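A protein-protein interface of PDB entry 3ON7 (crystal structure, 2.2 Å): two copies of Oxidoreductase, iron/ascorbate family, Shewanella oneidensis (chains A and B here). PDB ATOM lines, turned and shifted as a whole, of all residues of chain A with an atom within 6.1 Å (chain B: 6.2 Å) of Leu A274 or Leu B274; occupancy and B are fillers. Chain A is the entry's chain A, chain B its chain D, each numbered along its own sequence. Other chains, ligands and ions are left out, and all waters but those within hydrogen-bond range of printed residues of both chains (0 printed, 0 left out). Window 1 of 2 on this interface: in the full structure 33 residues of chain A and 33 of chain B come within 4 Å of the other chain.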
ATOM      1  N   TYR A 269      21.979  -3.680 -29.348  1.00  0.00           N
ATOM      2  CA  TYR A 269      20.685  -4.332 -29.510  1.00  0.00           C
ATOM      3  C   TYR A 269      20.672  -5.624 -28.689  1.00  0.00           C
ATOM      4  O   TYR A 269      19.719  -5.902 -27.998  1.00  0.00           O
ATOM      5  CB  TYR A 269      20.402  -4.661 -30.976  1.00  0.00           C
ATOM      6  CG  TYR A 269      18.994  -5.153 -31.207  1.00  0.00           C
ATOM      7  CD1 TYR A 269      17.959  -4.266 -31.470  1.00  0.00           C
ATOM      8  CD2 TYR A 269      18.691  -6.500 -31.171  1.00  0.00           C
ATOM      9  CE1 TYR A 269      16.662  -4.701 -31.677  1.00  0.00           C
ATOM     10  CE2 TYR A 269      17.386  -6.949 -31.377  1.00  0.00           C
ATOM     11  CZ  TYR A 269      16.381  -6.041 -31.625  1.00  0.00           C
ATOM     12  OH  TYR A 269      15.092  -6.469 -31.833  1.00  0.00           O
ATOM     13  N   LEU A 270      21.756  -6.387 -28.756  1.00  0.00           N
ATOM     14  CA  LEU A 270      21.864  -7.624 -27.969  1.00  0.00           C
ATOM     15  C   LEU A 270      21.912  -7.304 -26.473  1.00  0.00           C
ATOM     16  O   LEU A 270      21.180  -7.904 -25.701  1.00  0.00           O
ATOM     17  CB  LEU A 270      23.087  -8.464 -28.397  1.00  0.00           C
ATOM     18  CG  LEU A 270      23.389  -9.734 -27.596  1.00  0.00           C
ATOM     19  CD1 LEU A 270      22.183 -10.679 -27.601  1.00  0.00           C
ATOM     20  CD2 LEU A 270      24.624 -10.444 -28.120  1.00  0.00           C
ATOM     21  N   MET A 271      22.768  -6.370 -26.052  1.00  0.00           N
ATOM     22  CA  MET A 271      22.825  -6.033 -24.631  1.00  0.00           C
ATOM     23  C   MET A 271      21.435  -5.590 -24.170  1.00  0.00           C
ATOM     24  O   MET A 271      20.988  -5.990 -23.105  1.00  0.00           O
ATOM     25  CB  MET A 271      23.856  -4.927 -24.314  1.00  0.00           C
ATOM     26  CG  MET A 271      25.284  -5.252 -24.588  1.00  0.00           C
ATOM     27  SD  MET A 271      25.957  -6.711 -23.572  1.00  0.00           S
ATOM     28  CE  MET A 271      25.986  -8.126 -24.882  1.00  0.00           C
ATOM     29  N   GLU A 272      20.736  -4.783 -24.966  1.00  0.00           N
ATOM     30  CA  GLU A 272      19.416  -4.352 -24.549  1.00  0.00           C
ATOM     31  C   GLU A 272      18.474  -5.550 -24.329  1.00  0.00           C
ATOM     32  O   GLU A 272      17.682  -5.565 -23.371  1.00  0.00           O
ATOM     33  CB  GLU A 272      18.809  -3.362 -25.533  1.00  0.00           C
ATOM     34  CG  GLU A 272      17.452  -2.824 -25.098  1.00  0.00           C
ATOM     35  CD  GLU A 272      17.505  -2.067 -23.786  1.00  0.00           C
ATOM     36  OE1 GLU A 272      18.564  -1.465 -23.475  1.00  0.00           O
ATOM     37  OE2 GLU A 272      16.470  -2.070 -23.079  1.00  0.00           O
ATOM     38  N   ARG A 273      18.577  -6.552 -25.196  1.00  0.00           N
ATOM     39  CA  ARG A 273      17.773  -7.761 -25.044  1.00  0.00           C
ATOM     40  C   ARG A 273      18.133  -8.435 -23.736  1.00  0.00           C
ATOM     41  O   ARG A 273      17.252  -8.916 -23.022  1.00  0.00           O
ATOM     42  CB  ARG A 273      18.000  -8.748 -26.186  1.00  0.00           C
ATOM     43  CG  ARG A 273      17.134 -10.014 -26.115  1.00  0.00           C
ATOM     44  CD  ARG A 273      15.671  -9.694 -26.284  1.00  0.00           C
ATOM     45  NE  ARG A 273      15.386  -9.143 -27.615  1.00  0.00           N
ATOM     46  CZ  ARG A 273      15.148  -9.879 -28.701  1.00  0.00           C
ATOM     47  NH1 ARG A 273      15.140 -11.210 -28.648  1.00  0.00           N
ATOM     48  NH2 ARG A 273      14.903  -9.284 -29.859  1.00  0.00           N
ATOM     49  N   LEU A 274      19.417  -8.478 -23.415  1.00  0.00           N
ATOM     50  CA  LEU A 274      19.851  -9.133 -22.175  1.00  0.00           C
ATOM     51  C   LEU A 274      19.277  -8.455 -20.941  1.00  0.00           C
ATOM     52  O   LEU A 274      18.839  -9.128 -20.017  1.00  0.00           O
ATOM     53  CB  LEU A 274      21.371  -9.236 -22.107  1.00  0.00           C
ATOM     54  CG  LEU A 274      22.025 -10.156 -23.163  1.00  0.00           C
ATOM     55  CD1 LEU A 274      23.464 -10.394 -22.821  1.00  0.00           C
ATOM     56  CD2 LEU A 274      21.293 -11.503 -23.268  1.00  0.00           C
ATOM     57  N   ARG A 275      19.220  -7.127 -20.954  1.00  0.00           N
ATOM     58  CA  ARG A 275      18.606  -6.365 -19.870  1.00  0.00           C
ATOM     59  C   ARG A 275      17.083  -6.546 -19.826  1.00  0.00           C
ATOM     60  O   ARG A 275      16.509  -6.600 -18.731  1.00  0.00           O
ATOM     61  CB  ARG A 275      18.939  -4.863 -19.957  1.00  0.00           C
ATOM     62  CG  ARG A 275      20.413  -4.508 -20.167  1.00  0.00           C
ATOM     63  CD  ARG A 275      21.273  -4.750 -18.977  1.00  0.00           C
ATOM     64  NE  ARG A 275      21.549  -6.165 -18.771  1.00  0.00           N
ATOM     65  CZ  ARG A 275      22.546  -6.846 -19.327  1.00  0.00           C
ATOM     66  NH1 ARG A 275      23.398  -6.269 -20.182  1.00  0.00           N
ATOM     67  NH2 ARG A 275      22.693  -8.130 -19.028  1.00  0.00           N
ATOM     68  N   GLU A 276      16.426  -6.638 -20.986  1.00  0.00           N
ATOM     69  CA  GLU A 276      14.976  -6.926 -21.019  1.00  0.00           C
ATOM     70  C   GLU A 276      14.638  -8.291 -20.427  1.00  0.00           C
ATOM     71  O   GLU A 276      13.587  -8.468 -19.831  1.00  0.00           O
ATOM     72  CB  GLU A 276      14.434  -6.881 -22.456  1.00  0.00           C
ATOM     73  CG  GLU A 276      14.222  -5.444 -22.985  1.00  0.00           C
ATOM     74  CD  GLU A 276      13.832  -5.351 -24.475  1.00  0.00           C
ATOM     75  OE1 GLU A 276      13.967  -6.357 -25.226  1.00  0.00           O
ATOM     76  OE2 GLU A 276      13.400  -4.242 -24.888  1.00  0.00           O
ATOM     77  N   LEU A 277      15.524  -9.260 -20.618  1.00  0.00           N
ATOM     78  CA  LEU A 277      15.314 -10.601 -20.091  1.00  0.00           C
ATOM     79  C   LEU A 277      15.737 -10.689 -18.631  1.00  0.00           C
ATOM     80  O   LEU A 277      15.559 -11.720 -18.006  1.00  0.00           O
ATOM     81  CB  LEU A 277      16.095 -11.622 -20.905  1.00  0.00           C
ATOM     82  CG  LEU A 277      15.673 -11.845 -22.367  1.00  0.00           C
ATOM     83  CD1 LEU A 277      16.697 -12.681 -23.061  1.00  0.00           C
ATOM     84  CD2 LEU A 277      14.327 -12.511 -22.515  1.00  0.00           C
ATOM     85  N   GLY A 278      16.328  -9.621 -18.097  1.00  0.00           N
ATOM     86  CA  GLY A 278      16.793  -9.595 -16.709  1.00  0.00           C
ATOM     87  C   GLY A 278      18.004 -10.445 -16.388  1.00  0.00           C
ATOM     88  O   GLY A 278      18.203 -10.857 -15.239  1.00  0.00           O
ATOM     89  N   VAL A 279      18.818 -10.717 -17.396  1.00  0.00           N
ATOM     90  CA  VAL A 279      20.055 -11.462 -17.208  1.00  0.00           C
ATOM     91  C   VAL A 279      21.050 -10.586 -16.428  1.00  0.00           C
ATOM     92  O   VAL A 279      21.287  -9.438 -16.811  1.00  0.00           O
ATOM     93  CB  VAL A 279      20.687 -11.797 -18.589  1.00  0.00           C
ATOM     94  CG1 VAL A 279      22.110 -12.309 -18.427  1.00  0.00           C
ATOM     95  CG2 VAL A 279      19.785 -12.779 -19.386  1.00  0.00           C
ATOM     96  N   LEU A 280      21.641 -11.116 -15.361  1.00  0.00           N
ATOM     97  CA  LEU A 280      22.576 -10.329 -14.566  1.00  0.00           C
ATOM     98  C   LEU A 280      23.928 -10.068 -15.262  1.00  0.00           C
ATOM     99  O   LEU A 280      24.378 -10.779 -16.166  1.00  0.00           O
ATOM    100  CB  LEU A 280      22.784 -10.957 -13.170  1.00  0.00           C
ATOM    101  CG  LEU A 280      21.520 -11.072 -12.309  1.00  0.00           C
ATOM    102  CD1 LEU A 280      21.910 -11.420 -10.880  1.00  0.00           C
ATOM    103  CD2 LEU A 280      20.730  -9.801 -12.329  1.00  0.00           C
ATOM    104  OXT LEU A 280      24.608  -9.092 -14.910  1.00  0.00           O
ATOM    105  N   TYR B 269      16.245 -22.948 -18.574  1.00  0.00           N
ATOM    106  CA  TYR B 269      15.378 -22.266 -19.523  1.00  0.00           C
ATOM    107  C   TYR B 269      16.063 -20.973 -20.042  1.00  0.00           C
ATOM    108  O   TYR B 269      16.149 -20.710 -21.247  1.00  0.00           O
ATOM    109  CB  TYR B 269      14.007 -21.967 -18.874  1.00  0.00           C
ATOM    110  CG  TYR B 269      13.001 -21.482 -19.891  1.00  0.00           C
ATOM    111  CD1 TYR B 269      12.259 -22.376 -20.642  1.00  0.00           C
ATOM    112  CD2 TYR B 269      12.835 -20.130 -20.144  1.00  0.00           C
ATOM    113  CE1 TYR B 269      11.361 -21.940 -21.608  1.00  0.00           C
ATOM    114  CE2 TYR B 269      11.937 -19.690 -21.112  1.00  0.00           C
ATOM    115  CZ  TYR B 269      11.213 -20.595 -21.838  1.00  0.00           C
ATOM    116  OH  TYR B 269      10.324 -20.153 -22.783  1.00  0.00           O
ATOM    117  N   LEU B 270      16.565 -20.178 -19.119  1.00  0.00           N
ATOM    118  CA  LEU B 270      17.301 -18.978 -19.478  1.00  0.00           C
ATOM    119  C   LEU B 270      18.584 -19.343 -20.264  1.00  0.00           C
ATOM    120  O   LEU B 270      18.844 -18.798 -21.337  1.00  0.00           O
ATOM    121  CB  LEU B 270      17.624 -18.179 -18.218  1.00  0.00           C
ATOM    122  CG  LEU B 270      18.489 -16.934 -18.384  1.00  0.00           C
ATOM    123  CD1 LEU B 270      17.856 -16.002 -19.383  1.00  0.00           C
ATOM    124  CD2 LEU B 270      18.720 -16.286 -17.016  1.00  0.00           C
ATOM    125  N   MET B 271      19.352 -20.307 -19.774  1.00  0.00           N
ATOM    126  CA  MET B 271      20.540 -20.724 -20.501  1.00  0.00           C
ATOM    127  C   MET B 271      20.224 -21.058 -21.962  1.00  0.00           C
ATOM    128  O   MET B 271      20.890 -20.549 -22.852  1.00  0.00           O
ATOM    129  CB  MET B 271      21.241 -21.888 -19.807  1.00  0.00           C
ATOM    130  CG  MET B 271      21.965 -21.513 -18.500  1.00  0.00           C
ATOM    131  SD  MET B 271      23.197 -19.982 -18.619  1.00  0.00           S
ATOM    132  CE  MET B 271      22.194 -18.715 -17.637  1.00  0.00           C
ATOM    133  N   GLU B 272      19.197 -21.876 -22.203  1.00  0.00           N
ATOM    134  CA  GLU B 272      18.805 -22.275 -23.560  1.00  0.00           C
ATOM    135  C   GLU B 272      18.366 -21.078 -24.412  1.00  0.00           C
ATOM    136  O   GLU B 272      18.598 -21.041 -25.624  1.00  0.00           O
ATOM    137  CB  GLU B 272      17.654 -23.270 -23.472  1.00  0.00           C
ATOM    138  CG  GLU B 272      17.263 -23.929 -24.768  1.00  0.00           C
ATOM    139  CD  GLU B 272      18.332 -24.863 -25.282  1.00  0.00           C
ATOM    140  OE1 GLU B 272      19.132 -25.405 -24.468  1.00  0.00           O
ATOM    141  OE2 GLU B 272      18.358 -25.046 -26.517  1.00  0.00           O
ATOM    142  N   ARG B 273      17.728 -20.104 -23.780  1.00  0.00           N
ATOM    143  CA  ARG B 273      17.388 -18.866 -24.472  1.00  0.00           C
ATOM    144  C   ARG B 273      18.645 -18.229 -24.985  1.00  0.00           C
ATOM    145  O   ARG B 273      18.690 -17.853 -26.137  1.00  0.00           O
ATOM    146  CB  ARG B 273      16.628 -17.867 -23.575  1.00  0.00           C
ATOM    147  CG  ARG B 273      16.213 -16.589 -24.311  1.00  0.00           C
ATOM    148  CD  ARG B 273      15.267 -16.863 -25.489  1.00  0.00           C
ATOM    149  NE  ARG B 273      14.048 -17.509 -25.028  1.00  0.00           N
ATOM    150  CZ  ARG B 273      12.967 -16.861 -24.606  1.00  0.00           C
ATOM    151  NH1 ARG B 273      12.901 -15.538 -24.665  1.00  0.00           N
ATOM    152  NH2 ARG B 273      11.926 -17.549 -24.160  1.00  0.00           N
ATOM    153  N   LEU B 274      19.660 -18.113 -24.120  1.00  0.00           N
ATOM    154  CA  LEU B 274      20.948 -17.522 -24.501  1.00  0.00           C
ATOM    155  C   LEU B 274      21.683 -18.284 -25.607  1.00  0.00           C
ATOM    156  O   LEU B 274      22.296 -17.670 -26.479  1.00  0.00           O
ATOM    157  CB  LEU B 274      21.858 -17.388 -23.288  1.00  0.00           C
ATOM    158  CG  LEU B 274      21.294 -16.604 -22.087  1.00  0.00           C
ATOM    159  CD1 LEU B 274      22.360 -16.425 -20.982  1.00  0.00           C
ATOM    160  CD2 LEU B 274      20.695 -15.261 -22.536  1.00  0.00           C
ATOM    161  N   ARG B 275      21.626 -19.612 -25.582  1.00  0.00           N
ATOM    162  CA  ARG B 275      22.181 -20.394 -26.682  1.00  0.00           C
ATOM    163  C   ARG B 275      21.366 -20.152 -27.948  1.00  0.00           C
ATOM    164  O   ARG B 275      21.930 -20.056 -29.044  1.00  0.00           O
ATOM    165  CB  ARG B 275      22.252 -21.899 -26.370  1.00  0.00           C
ATOM    166  CG  ARG B 275      22.838 -22.257 -25.021  1.00  0.00           C
ATOM    167  CD  ARG B 275      24.314 -21.982 -24.871  1.00  0.00           C
ATOM    168  NE  ARG B 275      24.687 -20.565 -24.798  1.00  0.00           N
ATOM    169  CZ  ARG B 275      24.787 -19.832 -23.683  1.00  0.00           C
ATOM    170  NH1 ARG B 275      24.516 -20.322 -22.487  1.00  0.00           N
ATOM    171  NH2 ARG B 275      25.178 -18.575 -23.774  1.00  0.00           N
ATOM    172  N   GLU B 276      20.052 -20.026 -27.802  1.00  0.00           N
ATOM    173  CA  GLU B 276      19.212 -19.759 -28.950  1.00  0.00           C
ATOM    174  C   GLU B 276      19.531 -18.417 -29.602  1.00  0.00           C
ATOM    175  O   GLU B 276      19.458 -18.293 -30.805  1.00  0.00           O
ATOM    176  CB  GLU B 276      17.739 -19.813 -28.572  1.00  0.00           C
ATOM    177  CG  GLU B 276      17.132 -21.223 -28.574  1.00  0.00           C
ATOM    178  CD  GLU B 276      15.735 -21.250 -27.968  1.00  0.00           C
ATOM    179  OE1 GLU B 276      15.128 -20.167 -27.780  1.00  0.00           O
ATOM    180  OE2 GLU B 276      15.253 -22.363 -27.677  1.00  0.00           O
ATOM    181  N   LEU B 277      19.891 -17.427 -28.795  1.00  0.00           N
ATOM    182  CA  LEU B 277      20.212 -16.108 -29.299  1.00  0.00           C
ATOM    183  C   LEU B 277      21.653 -16.005 -29.801  1.00  0.00           C
ATOM    184  O   LEU B 277      22.012 -15.013 -30.408  1.00  0.00           O
ATOM    185  CB  LEU B 277      20.019 -15.067 -28.204  1.00  0.00           C
ATOM    186  CG  LEU B 277      18.667 -14.929 -27.528  1.00  0.00           C
ATOM    187  CD1 LEU B 277      18.841 -14.027 -26.299  1.00  0.00           C
ATOM    188  CD2 LEU B 277      17.664 -14.373 -28.482  1.00  0.00           C
ATOM    189  N   GLY B 278      22.485 -17.007 -29.531  1.00  0.00           N
ATOM    190  CA  GLY B 278      23.847 -17.017 -30.060  1.00  0.00           C
ATOM    191  C   GLY B 278      24.819 -16.225 -29.200  1.00  0.00           C
ATOM    192  O   GLY B 278      25.835 -15.781 -29.695  1.00  0.00           O
ATOM    193  N   VAL B 279      24.486 -16.039 -27.927  1.00  0.00           N
ATOM    194  CA  VAL B 279      25.324 -15.332 -26.966  1.00  0.00           C
ATOM    195  C   VAL B 279      26.515 -16.223 -26.559  1.00  0.00           C
ATOM    196  O   VAL B 279      26.326 -17.361 -26.106  1.00  0.00           O
ATOM    197  CB  VAL B 279      24.522 -15.010 -25.704  1.00  0.00           C
ATOM    198  CG1 VAL B 279      25.410 -14.448 -24.632  1.00  0.00           C
ATOM    199  CG2 VAL B 279      23.360 -14.078 -26.015  1.00  0.00           C
ATOM    200  N   LEU B 280      27.735 -15.727 -26.712  1.00  0.00           N
ATOM    201  CA  LEU B 280      28.906 -16.554 -26.396  1.00  0.00           C
ATOM    202  C   LEU B 280      29.130 -16.826 -24.883  1.00  0.00           C
ATOM    203  O   LEU B 280      28.703 -16.134 -23.951  1.00  0.00           O
ATOM    204  CB  LEU B 280      30.165 -15.982 -27.037  1.00  0.00           C
ATOM    205  CG  LEU B 280      30.071 -15.693 -28.538  1.00  0.00           C
ATOM    206  CD1 LEU B 280      31.423 -15.248 -29.065  1.00  0.00           C
ATOM    207  CD2 LEU B 280      29.608 -16.883 -29.299  1.00  0.00           C
ATOM    208  OXT LEU B 280      29.767 -17.823 -24.543  1.00  0.00           O
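Leu A274 touches just one residue of chain B: Leu B274. Of chain A, only Leu A274 comes within 4 Å of Leu B274. Printed residues of chain A within 4 Å of Arg B273: Leu A277. Of the printed residues of chain B, Leu A277 touches Arg B273 (3.98 Å). Printed residues of chain A within 4 Å of Val B279: Leu A270 (3.9 Å). Printed residues of chain A within 4 Å of Leu B270: Val A279. Tyr B269 touches none of the printed residues of chain A. Glu A272 touches none of the printed residues of chain B. The nearest residue of chain A that does not touch Leu B274 is Val A279 (4.1 Å).
The backbone carbonyl oxygen of Leu B274 lies within hydrogen-bond range of the backbone NH of Val B279. The backbone carbonyl oxygen (O) of Leu A274 is in hydrogen-bond range of the backbone NH (N) of Val A279. The guanidinium group of Arg A275 is in hydrogen-bond range of the backbone carbonyl oxygen of Val A279, at 2.9 Å. The guanidinium group (NH2) of Arg B273 sits at hydrogen-bond distance from the side-chain hydroxyl (OH) of Tyr B269. The guanidinium group (NH2) of Arg B275 sits at hydrogen-bond distance from the backbone carbonyl oxygen (O) of Val B279 (2.9 Å). NE of Arg B273 is in salt-bridge range of OE1 of Glu B276, 3.98 Å away.
Leu A270 touches Val B279. Leu A274 touches Leu B274. CD2 of Leu A277 touches NH1 of Arg B273 (3.98 Å). Val A279 touches Leu B270.
Leu A270 touches Val B279, and with the chains exchanged Val A279 touches Leu B270. Leu B274 touches its own counterpart, Leu A274. Leu A277 touches Arg B273, but with the chains exchanged Arg A273 does not touch Leu B277 (4.1 Å). Of the 4 pairs that touch across the chains among the printed residues, 3 have their exchanged pair printed and touching as well.
Of the 12 printed residues of chain A, 4 touch a printed residue of chain B. Along chain A the printed residues that touch a printed residue of chain B span positions 270 to 279. Of the 12 printed residues of chain B, 4 touch a printed residue of chain A. Hydrophobic or aromatic side chains of chain B that line the printed part of chain A: Leu B270, Leu B274 and Val B279. Among the printed residues, no Asp or Glu carboxylate lies within 4 Å of a Lys or Arg side-chain nitrogen of the other chain.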
